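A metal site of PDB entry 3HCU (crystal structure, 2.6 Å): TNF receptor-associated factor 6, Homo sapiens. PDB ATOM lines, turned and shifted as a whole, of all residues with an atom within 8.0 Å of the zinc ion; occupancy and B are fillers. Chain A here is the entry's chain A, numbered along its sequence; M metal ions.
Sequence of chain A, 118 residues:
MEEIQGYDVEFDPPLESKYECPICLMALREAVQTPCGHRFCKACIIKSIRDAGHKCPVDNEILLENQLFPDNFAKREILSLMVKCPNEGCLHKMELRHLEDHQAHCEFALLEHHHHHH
The zinc ion is bound by ND1 of His 38 (2.3 Å).
The side-chain sulfur (SG) of Cys 36 binds the zinc ion, 2.4 Å away.
SG of Cys 56 is bound to the zinc ion (2.5 Å).
OD1 of Asp 59 is bound to the zinc ion.
The zinc ion has four donor atoms within binding distance.
Of the 17 residues printed, 4 come within 4 Å of the zinc ion.
The side-chain hydroxyl (OG1) of Thr 34 sits at hydrogen-bond distance from the backbone NH (N) of His 38 (3.0 Å).
The side-chain hydroxyl (OG1) of Thr 34 lies close to the side-chain sulfur (SG) of Cys 36 (2.8 Å).
The side-chain sulfur (SG) of Cys 56 sits close to the backbone NH (N) of Val 58.
O of Glu 61 lies within hydrogen-bond range of N of Cys 56, at 2.7 Å.
The side-chain carboxylate of Asp 59 lies within hydrogen-bond range of the backbone NH of Glu 61 (3.0 Å).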
ATOM      1  N   THR A  34     -23.931  -4.831  23.731  1.00  0.00           N
ATOM      2  CA  THR A  34     -24.049  -5.941  22.822  1.00  0.00           C
ATOM      3  C   THR A  34     -23.305  -5.688  21.516  1.00  0.00           C
ATOM      4  O   THR A  34     -23.034  -4.543  21.171  1.00  0.00           O
ATOM      5  CB  THR A  34     -25.509  -6.177  22.482  1.00  0.00           C
ATOM      6  OG1 THR A  34     -26.008  -5.028  21.783  1.00  0.00           O
ATOM      7  CG2 THR A  34     -26.327  -6.401  23.731  1.00  0.00           C
ATOM      8  N   PRO A  35     -22.953  -6.754  20.786  1.00  0.00           N
ATOM      9  CA  PRO A  35     -22.239  -6.539  19.523  1.00  0.00           C
ATOM     10  C   PRO A  35     -22.977  -5.518  18.669  1.00  0.00           C
ATOM     11  O   PRO A  35     -22.377  -4.695  17.991  1.00  0.00           O
ATOM     12  CB  PRO A  35     -22.227  -7.940  18.886  1.00  0.00           C
ATOM     13  CG  PRO A  35     -22.097  -8.840  20.076  1.00  0.00           C
ATOM     14  CD  PRO A  35     -23.055  -8.199  21.099  1.00  0.00           C
ATOM     15  N   CYS A  36     -24.299  -5.587  18.709  1.00  0.00           N
ATOM     16  CA  CYS A  36     -25.153  -4.692  17.930  1.00  0.00           C
ATOM     17  C   CYS A  36     -25.204  -3.267  18.495  1.00  0.00           C
ATOM     18  O   CYS A  36     -25.950  -2.422  17.985  1.00  0.00           O
ATOM     19  CB  CYS A  36     -26.570  -5.274  17.840  1.00  0.00           C
ATOM     20  SG  CYS A  36     -27.272  -5.838  19.420  1.00  0.00           S
ATOM     21  N   GLY A  37     -24.450  -3.011  19.561  1.00  0.00           N
ATOM     22  CA  GLY A  37     -24.386  -1.670  20.129  1.00  0.00           C
ATOM     23  C   GLY A  37     -25.419  -1.179  21.120  1.00  0.00           C
ATOM     24  O   GLY A  37     -25.515   0.024  21.361  1.00  0.00           O
ATOM     25  N   HIS A  38     -26.194  -2.076  21.706  1.00  0.00           N
ATOM     26  CA  HIS A  38     -27.188  -1.664  22.677  1.00  0.00           C
ATOM     27  C   HIS A  38     -26.721  -1.960  24.076  1.00  0.00           C
ATOM     28  O   HIS A  38     -25.927  -2.874  24.303  1.00  0.00           O
ATOM     29  CB  HIS A  38     -28.515  -2.343  22.387  1.00  0.00           C
ATOM     30  CG  HIS A  38     -29.085  -1.937  21.077  1.00  0.00           C
ATOM     31  ND1 HIS A  38     -28.712  -2.533  19.887  1.00  0.00           N
ATOM     32  CD2 HIS A  38     -29.920  -0.931  20.747  1.00  0.00           C
ATOM     33  CE1 HIS A  38     -29.289  -1.906  18.884  1.00  0.00           C
ATOM     34  NE2 HIS A  38     -30.032  -0.924  19.373  1.00  0.00           N
ATOM     35  N   ARG A  39     -27.198  -1.149  25.010  1.00  0.00           N
ATOM     36  CA  ARG A  39     -26.822  -1.275  26.412  1.00  0.00           C
ATOM     37  C   ARG A  39     -27.988  -1.760  27.271  1.00  0.00           C
ATOM     38  O   ARG A  39     -29.151  -1.427  27.016  1.00  0.00           O
ATOM     39  CB  ARG A  39     -26.351   0.082  26.932  1.00  0.00           C
ATOM     40  CG  ARG A  39     -25.248   0.745  26.138  1.00  0.00           C
ATOM     41  CD  ARG A  39     -25.039   2.154  26.692  1.00  0.00           C
ATOM     42  NE  ARG A  39     -23.680   2.640  26.470  1.00  0.00           N
ATOM     43  CZ  ARG A  39     -23.215   3.048  25.297  1.00  0.00           C
ATOM     44  NH1 ARG A  39     -24.000   3.060  24.238  1.00  0.00           N
ATOM     45  NH2 ARG A  39     -21.944   3.418  25.183  1.00  0.00           N
ATOM     46  N   PHE A  40     -27.652  -2.545  28.288  1.00  0.00           N
ATOM     47  CA  PHE A  40     -28.605  -3.098  29.230  1.00  0.00           C
ATOM     48  C   PHE A  40     -27.927  -3.178  30.584  1.00  0.00           C
ATOM     49  O   PHE A  40     -26.731  -2.878  30.709  1.00  0.00           O
ATOM     50  CB  PHE A  40     -29.018  -4.537  28.836  1.00  0.00           C
ATOM     51  CG  PHE A  40     -29.675  -4.667  27.494  1.00  0.00           C
ATOM     52  CD1 PHE A  40     -28.953  -5.115  26.391  1.00  0.00           C
ATOM     53  CD2 PHE A  40     -31.011  -4.325  27.323  1.00  0.00           C
ATOM     54  CE1 PHE A  40     -29.552  -5.203  25.142  1.00  0.00           C
ATOM     55  CE2 PHE A  40     -31.610  -4.413  26.074  1.00  0.00           C
ATOM     56  CZ  PHE A  40     -30.868  -4.858  24.981  1.00  0.00           C
ATOM     57  N   ILE A  45     -30.033  -8.264  30.432  1.00  0.00           N
ATOM     58  CA  ILE A  45     -29.914  -8.917  29.153  1.00  0.00           C
ATOM     59  C   ILE A  45     -29.677 -10.418  29.338  1.00  0.00           C
ATOM     60  O   ILE A  45     -29.957 -11.217  28.433  1.00  0.00           O
ATOM     61  CB  ILE A  45     -28.833  -8.251  28.299  1.00  0.00           C
ATOM     62  CG1 ILE A  45     -29.066  -8.589  26.834  1.00  0.00           C
ATOM     63  CG2 ILE A  45     -27.464  -8.696  28.751  1.00  0.00           C
ATOM     64  CD1 ILE A  45     -30.425  -8.110  26.329  1.00  0.00           C
ATOM     65  N   LYS A  55     -31.503 -13.345  21.339  1.00  0.00           N
ATOM     66  CA  LYS A  55     -31.586 -12.224  20.418  1.00  0.00           C
ATOM     67  C   LYS A  55     -31.572 -10.934  21.228  1.00  0.00           C
ATOM     68  O   LYS A  55     -31.865 -10.930  22.425  1.00  0.00           O
ATOM     69  CB  LYS A  55     -32.855 -12.321  19.554  1.00  0.00           C
ATOM     70  CG  LYS A  55     -34.126 -12.654  20.295  1.00  0.00           C
ATOM     71  CD  LYS A  55     -35.296 -12.939  19.336  1.00  0.00           C
ATOM     72  CE  LYS A  55     -36.559 -13.323  20.102  1.00  0.00           C
ATOM     73  NZ  LYS A  55     -37.732 -13.664  19.230  1.00  0.00           N
ATOM     74  N   CYS A  56     -31.160  -9.849  20.604  1.00  0.00           N
ATOM     75  CA  CYS A  56     -31.147  -8.582  21.322  1.00  0.00           C
ATOM     76  C   CYS A  56     -32.595  -8.107  21.291  1.00  0.00           C
ATOM     77  O   CYS A  56     -33.222  -8.063  20.237  1.00  0.00           O
ATOM     78  CB  CYS A  56     -30.256  -7.559  20.628  1.00  0.00           C
ATOM     79  SG  CYS A  56     -30.512  -5.885  21.233  1.00  0.00           S
ATOM     80  N   PRO A  57     -33.153  -7.770  22.457  1.00  0.00           N
ATOM     81  CA  PRO A  57     -34.539  -7.321  22.464  1.00  0.00           C
ATOM     82  C   PRO A  57     -34.792  -6.083  21.611  1.00  0.00           C
ATOM     83  O   PRO A  57     -35.889  -5.897  21.087  1.00  0.00           O
ATOM     84  CB  PRO A  57     -34.807  -7.064  23.944  1.00  0.00           C
ATOM     85  CG  PRO A  57     -33.470  -6.667  24.457  1.00  0.00           C
ATOM     86  CD  PRO A  57     -32.527  -7.610  23.780  1.00  0.00           C
ATOM     87  N   VAL A  58     -33.778  -5.249  21.423  1.00  0.00           N
ATOM     88  CA  VAL A  58     -33.957  -4.044  20.636  1.00  0.00           C
ATOM     89  C   VAL A  58     -34.122  -4.244  19.136  1.00  0.00           C
ATOM     90  O   VAL A  58     -34.682  -3.375  18.466  1.00  0.00           O
ATOM     91  CB  VAL A  58     -32.780  -3.054  20.823  1.00  0.00           C
ATOM     92  CG1 VAL A  58     -33.051  -1.798  20.052  1.00  0.00           C
ATOM     93  CG2 VAL A  58     -32.552  -2.731  22.294  1.00  0.00           C
ATOM     94  N   ASP A  59     -33.660  -5.361  18.588  1.00  0.00           N
ATOM     95  CA  ASP A  59     -33.752  -5.556  17.145  1.00  0.00           C
ATOM     96  C   ASP A  59     -33.804  -7.026  16.693  1.00  0.00           C
ATOM     97  O   ASP A  59     -33.628  -7.332  15.503  1.00  0.00           O
ATOM     98  CB  ASP A  59     -32.582  -4.848  16.476  1.00  0.00           C
ATOM     99  CG  ASP A  59     -31.257  -5.294  17.038  1.00  0.00           C
ATOM    100  OD1 ASP A  59     -30.279  -4.515  16.995  1.00  0.00           O
ATOM    101  OD2 ASP A  59     -31.189  -6.443  17.506  1.00  0.00           O
ATOM    102  N   ASN A  60     -34.020  -7.926  17.644  1.00  0.00           N
ATOM    103  CA  ASN A  60     -34.101  -9.348  17.369  1.00  0.00           C
ATOM    104  C   ASN A  60     -32.882  -9.960  16.700  1.00  0.00           C
ATOM    105  O   ASN A  60     -32.937 -11.054  16.172  1.00  0.00           O
ATOM    106  CB  ASN A  60     -35.357  -9.632  16.536  1.00  0.00           C
ATOM    107  CG  ASN A  60     -36.626  -9.583  17.372  1.00  0.00           C
ATOM    108  OD1 ASN A  60     -37.740  -9.527  16.850  1.00  0.00           O
ATOM    109  ND2 ASN A  60     -36.459  -9.625  18.707  1.00  0.00           N
ATOM    110  N   GLU A  61     -31.766  -9.245  16.749  1.00  0.00           N
ATOM    111  CA  GLU A  61     -30.518  -9.730  16.161  1.00  0.00           C
ATOM    112  C   GLU A  61     -29.903 -10.765  17.119  1.00  0.00           C
ATOM    113  O   GLU A  61     -29.939 -10.588  18.336  1.00  0.00           O
ATOM    114  CB  GLU A  61     -29.547  -8.563  15.973  1.00  0.00           C
ATOM    115  CG  GLU A  61     -28.428  -8.816  14.999  1.00  0.00           C
ATOM    116  CD  GLU A  61     -27.174  -8.054  15.356  1.00  0.00           C
ATOM    117  OE1 GLU A  61     -26.548  -8.396  16.396  1.00  0.00           O
ATOM    118  OE2 GLU A  61     -26.806  -7.110  14.616  1.00  0.00           O
ATOM    119  N   ILE A  62     -29.360 -11.840  16.566  1.00  0.00           N
ATOM    120  CA  ILE A  62     -28.761 -12.886  17.385  1.00  0.00           C
ATOM    121  C   ILE A  62     -27.833 -12.247  18.402  1.00  0.00           C
ATOM    122  O   ILE A  62     -27.036 -11.392  18.042  1.00  0.00           O
ATOM    123  CB  ILE A  62     -27.942 -13.890  16.542  1.00  0.00           C
ATOM    124  CG1 ILE A  62     -28.737 -14.358  15.313  1.00  0.00           C
ATOM    125  CG2 ILE A  62     -27.586 -15.091  17.397  1.00  0.00           C
ATOM    126  CD1 ILE A  62     -29.980 -15.178  15.635  1.00  0.00           C
ATOM    127  N   LEU A  63     -27.925 -12.666  19.659  1.00  0.00           N
ATOM    128  CA  LEU A  63     -27.082 -12.087  20.697  1.00  0.00           C
ATOM    129  C   LEU A  63     -26.073 -13.024  21.371  1.00  0.00           C
ATOM    130  O   LEU A  63     -24.866 -12.836  21.202  1.00  0.00           O
ATOM    131  CB  LEU A  63     -27.926 -11.380  21.772  1.00  0.00           C
ATOM    132  CG  LEU A  63     -27.151 -10.764  22.945  1.00  0.00           C
ATOM    133  CD1 LEU A  63     -25.974  -9.962  22.455  1.00  0.00           C
ATOM    134  CD2 LEU A  63     -28.070  -9.894  23.754  1.00  0.00           C
HETATM  135 ZN    ZN M   1     -29.333  -4.673  19.365  1.00  0.00          ZN
